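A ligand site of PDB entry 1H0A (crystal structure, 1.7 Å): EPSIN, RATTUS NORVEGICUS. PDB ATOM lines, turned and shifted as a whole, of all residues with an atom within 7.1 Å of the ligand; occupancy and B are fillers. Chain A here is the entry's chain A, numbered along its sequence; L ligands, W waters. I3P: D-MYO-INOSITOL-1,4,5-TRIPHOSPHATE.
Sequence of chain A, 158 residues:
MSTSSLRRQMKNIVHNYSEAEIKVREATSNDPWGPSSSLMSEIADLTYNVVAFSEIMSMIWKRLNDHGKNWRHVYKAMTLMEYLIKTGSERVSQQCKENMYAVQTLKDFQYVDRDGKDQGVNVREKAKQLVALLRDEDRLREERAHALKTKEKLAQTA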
ATOM      1  N   SER A   4      -1.547  -6.788 -23.355  1.00  0.00           N
ATOM      2  CA  SER A   4      -2.400  -7.907 -23.816  1.00  0.00           C
ATOM      3  C   SER A   4      -1.486  -8.894 -24.480  1.00  0.00           C
ATOM      4  O   SER A   4      -1.639 -10.068 -24.234  1.00  0.00           O
ATOM      5  CB  SER A   4      -3.600  -7.467 -24.765  1.00  0.00           C
ATOM      6  OG  SER A   4      -3.145  -7.101 -26.099  1.00  0.00           O
ATOM      7  N   SER A   5      -0.536  -8.437 -25.303  1.00  0.00           N
ATOM      8  CA  SER A   5       0.473  -9.286 -25.925  1.00  0.00           C
ATOM      9  C   SER A   5       1.307 -10.098 -24.979  1.00  0.00           C
ATOM     10  O   SER A   5       1.507 -11.315 -25.133  1.00  0.00           O
ATOM     11  CB  SER A   5       1.357  -8.430 -26.794  1.00  0.00           C
ATOM     12  OG  SER A   5       2.266  -9.259 -27.450  1.00  0.00           O
ATOM     13  N   ARG A   7       0.427 -11.036 -21.850  1.00  0.00           N
ATOM     14  CA  ARG A   7      -0.356 -12.074 -21.238  1.00  0.00           C
ATOM     15  C   ARG A   7      -0.576 -13.238 -22.215  1.00  0.00           C
ATOM     16  O   ARG A   7      -0.637 -14.366 -21.768  1.00  0.00           O
ATOM     17  CB  ARG A   7      -1.759 -11.556 -20.818  1.00  0.00           C
ATOM     18  CG  ARG A   7      -1.810 -10.742 -19.594  1.00  0.00           C
ATOM     19  CD  ARG A   7      -3.146 -10.416 -19.152  1.00  0.00           C
ATOM     20  NE  ARG A   7      -3.817 -11.566 -18.609  1.00  0.00           N
ATOM     21  CZ  ARG A   7      -5.171 -11.665 -18.592  1.00  0.00           C
ATOM     22  NH1 ARG A   7      -5.866 -10.690 -19.148  1.00  0.00           N
ATOM     23  NH2 ARG A   7      -5.809 -12.710 -18.125  1.00  0.00           N
ATOM     24  N   ARG A   8      -0.838 -12.890 -23.469  1.00  0.00           N
ATOM     25  CA  ARG A   8      -1.022 -13.891 -24.546  1.00  0.00           C
ATOM     26  C   ARG A   8       0.177 -14.836 -24.675  1.00  0.00           C
ATOM     27  O   ARG A   8       0.032 -16.060 -24.657  1.00  0.00           O
ATOM     28  CB  ARG A   8      -1.389 -13.180 -25.852  1.00  0.00           C
ATOM     29  CG  ARG A   8      -1.723 -14.032 -27.050  1.00  0.00           C
ATOM     30  CD  ARG A   8      -2.062 -13.194 -28.350  1.00  0.00           C
ATOM     31  NE  ARG A   8      -2.935 -12.203 -28.006  1.00  0.00           N
ATOM     32  CZ  ARG A   8      -2.784 -10.896 -28.186  1.00  0.00           C
ATOM     33  NH1 ARG A   8      -1.789 -10.410 -28.922  1.00  0.00           N
ATOM     34  NH2 ARG A   8      -3.655 -10.121 -27.605  1.00  0.00           N
ATOM     35  N   GLN A   9       1.384 -14.230 -24.629  1.00  0.00           N
ATOM     36  CA  GLN A   9       2.605 -14.992 -24.675  1.00  0.00           C
ATOM     37  C   GLN A   9       2.887 -15.854 -23.462  1.00  0.00           C
ATOM     38  O   GLN A   9       3.336 -16.973 -23.571  1.00  0.00           O
ATOM     39  CB  GLN A   9       3.745 -14.025 -24.842  1.00  0.00           C
ATOM     40  CG  GLN A   9       3.754 -13.411 -26.140  1.00  0.00           C
ATOM     41  CD  GLN A   9       4.923 -12.482 -26.250  1.00  0.00           C
ATOM     42  OE1 GLN A   9       6.056 -12.929 -26.132  1.00  0.00           O
ATOM     43  NE2 GLN A   9       4.659 -11.182 -26.200  1.00  0.00           N
ATOM     44  N   LYS A  11       0.551 -17.122 -21.609  1.00  0.00           N
ATOM     45  CA  LYS A  11      -0.399 -18.217 -21.810  1.00  0.00           C
ATOM     46  C   LYS A  11       0.192 -19.261 -22.790  1.00  0.00           C
ATOM     47  O   LYS A  11       0.049 -20.515 -22.574  1.00  0.00           O
ATOM     48  CB  LYS A  11      -1.840 -17.726 -22.232  1.00  0.00           C
ATOM     49  CG  LYS A  11      -2.798 -18.855 -22.337  1.00  0.00           C
ATOM     50  CD  LYS A  11      -4.245 -18.428 -22.675  1.00  0.00           C
ATOM     51  CE  LYS A  11      -5.185 -19.571 -22.690  1.00  0.00           C
ATOM     52  NZ  LYS A  11      -6.618 -19.251 -22.325  1.00  0.00           N
ATOM     53  N   ASN A  12       0.807 -18.787 -23.861  1.00  0.00           N
ATOM     54  CA  ASN A  12       1.446 -19.641 -24.836  1.00  0.00           C
ATOM     55  C   ASN A  12       2.494 -20.510 -24.238  1.00  0.00           C
ATOM     56  O   ASN A  12       2.615 -21.715 -24.496  1.00  0.00           O
ATOM     57  CB  ASN A  12       2.001 -18.791 -25.926  1.00  0.00           C
ATOM     58  CG  ASN A  12       0.835 -18.191 -26.844  1.00  0.00           C
ATOM     59  OD1 ASN A  12      -0.315 -18.557 -26.606  1.00  0.00           O
ATOM     60  ND2 ASN A  12       1.125 -17.241 -27.664  1.00  0.00           N
ATOM     61  N   TYR A  17       1.990 -24.189 -26.428  1.00  0.00           N
ATOM     62  CA  TYR A  17       1.343 -24.153 -27.718  1.00  0.00           C
ATOM     63  C   TYR A  17       2.393 -24.168 -28.804  1.00  0.00           C
ATOM     64  O   TYR A  17       3.487 -23.521 -28.729  1.00  0.00           O
ATOM     65  CB  TYR A  17       0.464 -22.919 -27.901  1.00  0.00           C
ATOM     66  CG  TYR A  17      -0.902 -22.979 -27.133  1.00  0.00           C
ATOM     67  CD1 TYR A  17      -1.417 -21.802 -26.557  1.00  0.00           C
ATOM     68  CD2 TYR A  17      -1.593 -24.154 -26.957  1.00  0.00           C
ATOM     69  CE1 TYR A  17      -2.586 -21.806 -25.833  1.00  0.00           C
ATOM     70  CE2 TYR A  17      -2.780 -24.164 -26.235  1.00  0.00           C
ATOM     71  CZ  TYR A  17      -3.269 -22.965 -25.684  1.00  0.00           C
ATOM     72  OH  TYR A  17      -4.480 -22.873 -24.992  1.00  0.00           O
ATOM     73  N   ARG A  25      -3.895 -17.972 -32.445  1.00  0.00           N
ATOM     74  CA  ARG A  25      -4.256 -17.139 -31.286  1.00  0.00           C
ATOM     75  C   ARG A  25      -4.063 -15.710 -31.469  1.00  0.00           C
ATOM     76  O   ARG A  25      -4.843 -14.870 -31.088  1.00  0.00           O
ATOM     77  CB  ARG A  25      -3.635 -17.672 -29.955  1.00  0.00           C
ATOM     78  CG  ARG A  25      -4.423 -18.907 -29.327  1.00  0.00           C
ATOM     79  CD  ARG A  25      -3.610 -19.764 -28.327  1.00  0.00           C
ATOM     80  NE  ARG A  25      -2.986 -18.789 -27.391  1.00  0.00           N
ATOM     81  CZ  ARG A  25      -3.631 -18.080 -26.474  1.00  0.00           C
ATOM     82  NH1 ARG A  25      -4.922 -18.162 -26.290  1.00  0.00           N
ATOM     83  NH2 ARG A  25      -2.964 -17.248 -25.664  1.00  0.00           N
ATOM     84  N   GLU A  26      -2.951 -15.357 -32.144  1.00  0.00           N
ATOM     85  CA  GLU A  26      -2.726 -13.991 -32.423  1.00  0.00           C
ATOM     86  C   GLU A  26      -3.705 -13.410 -33.425  1.00  0.00           C
ATOM     87  O   GLU A  26      -4.300 -12.354 -33.230  1.00  0.00           O
ATOM     88  CB  GLU A  26      -1.285 -13.855 -32.925  1.00  0.00           C
ATOM     89  CG  GLU A  26      -0.881 -12.473 -33.345  1.00  0.00           C
ATOM     90  CD  GLU A  26      -0.872 -11.448 -32.194  1.00  0.00           C
ATOM     91  OE1 GLU A  26      -1.277 -10.266 -32.448  1.00  0.00           O
ATOM     92  OE2 GLU A  26      -0.433 -11.867 -31.070  1.00  0.00           O
ATOM     93  N   THR A  28      -6.707 -14.309 -33.914  1.00  0.00           N
ATOM     94  CA  THR A  28      -8.030 -14.307 -33.389  1.00  0.00           C
ATOM     95  C   THR A  28      -8.206 -13.649 -32.039  1.00  0.00           C
ATOM     96  O   THR A  28      -9.160 -13.929 -31.286  1.00  0.00           O
ATOM     97  CB  THR A  28      -8.619 -15.734 -33.429  1.00  0.00           C
ATOM     98  OG1 THR A  28      -7.869 -16.625 -32.537  1.00  0.00           O
ATOM     99  CG2 THR A  28      -8.539 -16.315 -34.835  1.00  0.00           C
ATOM    100  N   SER A  29      -7.239 -12.822 -31.667  1.00  0.00           N
ATOM    101  CA  SER A  29      -7.252 -12.196 -30.353  1.00  0.00           C
ATOM    102  C   SER A  29      -8.425 -11.195 -30.155  1.00  0.00           C
ATOM    103  O   SER A  29      -9.082 -10.710 -31.141  1.00  0.00           O
ATOM    104  CB  SER A  29      -5.938 -11.512 -30.151  1.00  0.00           C
ATOM    105  OG  SER A  29      -5.863 -10.268 -30.857  1.00  0.00           O
ATOM    106  N   ASN A  30      -8.644 -10.782 -28.877  1.00  0.00           N
ATOM    107  CA  ASN A  30      -9.550  -9.742 -28.499  1.00  0.00           C
ATOM    108  C   ASN A  30      -9.061  -8.364 -28.894  1.00  0.00           C
ATOM    109  O   ASN A  30      -9.754  -7.368 -28.672  1.00  0.00           O
ATOM    110  CB  ASN A  30      -9.906  -9.778 -26.990  1.00  0.00           C
ATOM    111  CG  ASN A  30     -10.917 -10.736 -26.643  1.00  0.00           C
ATOM    112  OD1 ASN A  30     -11.785 -11.060 -27.504  1.00  0.00           O
ATOM    113  ND2 ASN A  30     -10.912 -11.201 -25.387  1.00  0.00           N
ATOM    114  N   ASP A  31      -7.926  -8.231 -29.534  1.00  0.00           N
ATOM    115  CA  ASP A  31      -7.488  -6.894 -29.916  1.00  0.00           C
ATOM    116  C   ASP A  31      -8.427  -6.291 -30.984  1.00  0.00           C
ATOM    117  O   ASP A  31      -8.861  -7.008 -31.869  1.00  0.00           O
ATOM    118  CB  ASP A  31      -6.087  -6.844 -30.451  1.00  0.00           C
ATOM    119  CG  ASP A  31      -4.970  -7.160 -29.330  1.00  0.00           C
ATOM    120  OD1 ASP A  31      -5.163  -6.959 -28.086  1.00  0.00           O
ATOM    121  OD2 ASP A  31      -3.865  -7.616 -29.658  1.00  0.00           O
ATOM    122  N   ARG A  63     -12.019 -21.081 -30.434  1.00  0.00           N
ATOM    123  CA  ARG A  63     -12.290 -19.678 -30.473  1.00  0.00           C
ATOM    124  C   ARG A  63     -13.745 -19.353 -30.895  1.00  0.00           C
ATOM    125  O   ARG A  63     -14.390 -18.440 -30.307  1.00  0.00           O
ATOM    126  CB  ARG A  63     -11.290 -18.926 -31.379  1.00  0.00           C
ATOM    127  CG  ARG A  63      -9.991 -18.814 -30.762  1.00  0.00           C
ATOM    128  CD  ARG A  63      -9.933 -17.562 -29.985  1.00  0.00           C
ATOM    129  NE  ARG A  63      -9.121 -17.496 -28.784  1.00  0.00           N
ATOM    130  CZ  ARG A  63      -8.098 -16.783 -28.675  1.00  0.00           C
ATOM    131  NH1 ARG A  63      -7.554 -16.242 -29.711  1.00  0.00           N
ATOM    132  NH2 ARG A  63      -7.535 -16.698 -27.526  1.00  0.00           N
ATOM    133  N   ASP A  66     -16.371 -19.333 -27.997  1.00  0.00           N
ATOM    134  CA  ASP A  66     -16.325 -18.325 -26.957  1.00  0.00           C
ATOM    135  C   ASP A  66     -17.639 -17.528 -26.851  1.00  0.00           C
ATOM    136  O   ASP A  66     -18.589 -17.694 -27.668  1.00  0.00           O
ATOM    137  CB  ASP A  66     -15.136 -17.403 -27.137  1.00  0.00           C
ATOM    138  CG  ASP A  66     -14.444 -17.126 -25.827  1.00  0.00           C
ATOM    139  OD1 ASP A  66     -15.146 -17.097 -24.751  1.00  0.00           O
ATOM    140  OD2 ASP A  66     -13.200 -16.960 -25.842  1.00  0.00           O
ATOM    141  N   LYS A  69     -18.229 -11.147 -23.713  1.00  0.00           N
ATOM    142  CA  LYS A  69     -17.280 -10.103 -23.972  1.00  0.00           C
ATOM    143  C   LYS A  69     -16.087 -10.535 -24.858  1.00  0.00           C
ATOM    144  O   LYS A  69     -15.346  -9.705 -25.254  1.00  0.00           O
ATOM    145  CB  LYS A  69     -16.748  -9.564 -22.649  1.00  0.00           C
ATOM    146  CG  LYS A  69     -16.121 -10.638 -21.786  1.00  0.00           C
ATOM    147  CD  LYS A  69     -14.669 -10.563 -21.952  1.00  0.00           C
ATOM    148  CE  LYS A  69     -13.960 -11.360 -20.869  1.00  0.00           C
ATOM    149  NZ  LYS A  69     -12.533 -11.641 -21.210  1.00  0.00           N
ATOM    150  N   ASN A  70     -15.918 -11.822 -25.082  1.00  0.00           N
ATOM    151  CA  ASN A  70     -14.888 -12.370 -25.950  1.00  0.00           C
ATOM    152  C   ASN A  70     -15.450 -12.552 -27.413  1.00  0.00           C
ATOM    153  O   ASN A  70     -14.937 -13.379 -28.170  1.00  0.00           O
ATOM    154  CB  ASN A  70     -14.424 -13.729 -25.421  1.00  0.00           C
ATOM    155  CG  ASN A  70     -13.580 -13.627 -24.144  1.00  0.00           C
ATOM    156  OD1 ASN A  70     -12.878 -12.647 -23.930  1.00  0.00           O
ATOM    157  ND2 ASN A  70     -13.609 -14.702 -23.346  1.00  0.00           N
ATOM    158  N   HIS A  73     -13.144 -12.946 -30.454  1.00  0.00           N
ATOM    159  CA  HIS A  73     -12.592 -14.263 -30.662  1.00  0.00           C
ATOM    160  C   HIS A  73     -13.424 -14.997 -31.792  1.00  0.00           C
ATOM    161  O   HIS A  73     -12.855 -15.600 -32.650  1.00  0.00           O
ATOM    162  CB  HIS A  73     -12.657 -15.115 -29.445  1.00  0.00           C
ATOM    163  CG  HIS A  73     -11.584 -14.718 -28.443  1.00  0.00           C
ATOM    164  ND1 HIS A  73     -11.491 -15.279 -27.184  1.00  0.00           N
ATOM    165  CD2 HIS A  73     -10.517 -13.909 -28.593  1.00  0.00           C
ATOM    166  CE1 HIS A  73     -10.452 -14.721 -26.538  1.00  0.00           C
ATOM    167  NE2 HIS A  73      -9.813 -13.907 -27.375  1.00  0.00           N
ATOM    168  N   LYS A  76     -13.317 -12.981 -35.287  1.00  0.00           N
ATOM    169  CA  LYS A  76     -12.074 -13.137 -35.956  1.00  0.00           C
ATOM    170  C   LYS A  76     -11.767 -14.596 -36.416  1.00  0.00           C
ATOM    171  O   LYS A  76     -11.000 -14.804 -37.378  1.00  0.00           O
ATOM    172  CB  LYS A  76     -10.899 -12.503 -35.132  1.00  0.00           C
ATOM    173  CG  LYS A  76     -11.109 -11.069 -35.033  1.00  0.00           C
ATOM    174  CD  LYS A  76     -10.100 -10.323 -34.003  1.00  0.00           C
ATOM    175  CE  LYS A  76      -8.807  -9.967 -34.467  1.00  0.00           C
ATOM    176  NZ  LYS A  76      -8.030  -9.334 -33.281  1.00  0.00           N
HETATM  177  C1  I3P L   1      -8.838 -12.596 -21.147  1.00  0.00           C
HETATM  178  C2  I3P L   1      -8.643 -11.345 -22.006  1.00  0.00           C
HETATM  179  C3  I3P L   1      -7.523 -11.546 -23.009  1.00  0.00           C
HETATM  180  C4  I3P L   1      -7.809 -12.771 -23.846  1.00  0.00           C
HETATM  181  C5  I3P L   1      -8.090 -14.004 -23.050  1.00  0.00           C
HETATM  182  C6  I3P L   1      -9.138 -13.867 -21.889  1.00  0.00           C
HETATM  183  O1  I3P L   1      -9.970 -12.469 -20.194  1.00  0.00           O
HETATM  184  O2  I3P L   1      -9.824 -10.881 -22.700  1.00  0.00           O
HETATM  185  O3  I3P L   1      -7.391 -10.332 -23.735  1.00  0.00           O
HETATM  186  O4  I3P L   1      -6.694 -13.069 -24.649  1.00  0.00           O
HETATM  187  O5  I3P L   1      -8.532 -15.007 -23.999  1.00  0.00           O
HETATM  188  O6  I3P L   1      -9.342 -15.052 -21.083  1.00  0.00           O
HETATM  189  P1  I3P L   1      -9.498 -11.893 -18.718  1.00  0.00           P
HETATM  190  O11 I3P L   1      -8.735 -12.974 -18.141  1.00  0.00           O
HETATM  191  O12 I3P L   1     -10.860 -11.740 -18.137  1.00  0.00           O
HETATM  192  O13 I3P L   1      -8.750 -10.695 -18.808  1.00  0.00           O
HETATM  193  P4  I3P L   1      -6.279 -12.451 -26.076  1.00  0.00           P
HETATM  194  O41 I3P L   1      -7.582 -12.368 -26.942  1.00  0.00           O
HETATM  195  O42 I3P L   1      -5.798 -11.072 -25.846  1.00  0.00           O
HETATM  196  O43 I3P L   1      -5.358 -13.456 -26.530  1.00  0.00           O
HETATM  197  P5  I3P L   1      -8.122 -16.514 -24.016  1.00  0.00           P
HETATM  198  O51 I3P L   1      -8.985 -17.333 -24.946  1.00  0.00           O
HETATM  199  O52 I3P L   1      -8.589 -17.160 -22.716  1.00  0.00           O
HETATM  200  O53 I3P L   1      -6.665 -16.664 -24.379  1.00  0.00           O
HETATM  201  O   HOH W   1     -10.463 -18.855 -27.041  1.00  0.00           O
HETATM  202  O   HOH W   2      -8.247  -7.173 -24.766  1.00  0.00           O
HETATM  203  O   HOH W   3     -12.509 -13.842 -18.163  1.00  0.00           O
HETATM  204  O   HOH W   4     -12.246 -14.814 -20.886  1.00  0.00           O
HETATM  205  O   HOH W   5      -4.163 -13.668 -22.387  1.00  0.00           O
HETATM  206  O   HOH W   6      -5.589 -15.180 -28.280  1.00  0.00           O
HETATM  207  O   HOH W   7     -11.874 -17.589 -23.597  1.00  0.00           O
HETATM  208  O   HOH W   8      -4.539 -15.198 -24.586  1.00  0.00           O
HETATM  209  O   HOH W   9     -10.337  -8.430 -23.726  1.00  0.00           O
HETATM  210  O   HOH W  10      -4.186 -11.082 -23.472  1.00  0.00           O
HETATM  211  O   HOH W  11     -12.082  -9.112 -21.671  1.00  0.00           O
HETATM  212  O   HOH W  12      -6.772  -8.578 -26.458  1.00  0.00           O
HETATM  213  O   HOH W  13      -5.237  -9.236 -21.513  1.00  0.00           O
HETATM  214  O   HOH W  14      -7.496  -7.936 -21.923  1.00  0.00           O
HETATM  215  O   HOH W  15      -9.456  -8.357 -20.282  1.00  0.00           O
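Water W6 lies within hydrogen-bond range of O43 of the ligand (2.5 Å), NH2 of Arg 63 (2.6 Å) and O of Arg 25 (2.9 Å).
Water W8 bridges O53 of the ligand and NH2 of Arg 25.
Water W12 bridges O42 of the ligand (2.7 Å) and OD1 of Asp 31 (2.8 Å).
Water W4 lies within hydrogen-bond range of ND2 of Asn 70, O6 of the ligand and NZ of Lys 69.
Water W11 bridges NZ of Lys 69 (2.6 Å) and O2 of the ligand (3.0 Å).
Water W13 lies within hydrogen-bond range of the guanidinium group of Arg 7 and an oxygen (O3) of the ligand.
The side-chain amide oxygen of Asn 30 sits close to a ring nitrogen (NE2) of His 73 (3.5 Å).
The side-chain amino group (NZ) of Lys 69 sits at hydrogen-bond distance from the side-chain amide oxygen (OD1) of Asn 70 (2.9 Å).
OD2 of Asp 66 sits at hydrogen-bond distance from ND1 of His 73 (2.7 Å).
OD2 of Asp 31 lies within salt-bridge range of NH2 of Arg 8, 3.2 Å away.
OD1 of Asp 66 sits at hydrogen-bond distance from ND2 of Asn 70.
O of Arg 8 lies close to OD1 of Asn 12 (3.2 Å).
The side-chain hydroxyl of Ser 29 lies close to the backbone NH of Asp 31 (3.2 Å).
The guanidinium group (NH1) of Arg 63 lies within hydrogen-bond range of the side-chain hydroxyl (OG1) of Thr 28.
The side-chain amino group (NZ) of Lys 69 lies within salt-bridge range of an oxygen (O12) of the ligand, 3.5 Å away.
An oxygen (O51) of the ligand is in salt-bridge range of the guanidinium group (NH2) of Arg 63 (3.0 Å).
The side-chain amide nitrogen of Asn 30 lies within hydrogen-bond range of an oxygen (O2) of the ligand.
The guanidinium group (NH1) of Arg 7 is in salt-bridge range of an oxygen (O13) of the ligand (2.9 Å).
An oxygen (O42) of the ligand lies within salt-bridge range of the guanidinium group (NH2) of Arg 8 (2.9 Å).
O52 of the ligand lies within salt-bridge range of NZ of Lys 11 (2.9 Å).
The guanidinium group (NH1) of Arg 25 lies within salt-bridge range of an oxygen (O53) of the ligand (3.0 Å).
A ring nitrogen (NE2) of His 73 lies within hydrogen-bond range of an oxygen (O41) of the ligand, 2.7 Å away.
N of Asn 30 lies within hydrogen-bond range of O41 of the ligand (2.7 Å).
Ser 29 touches the ligand.
Asn 70 touches the ligand.
The nearest printed residue that does not touch the ligand is Asp 66 (4.3 Å).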
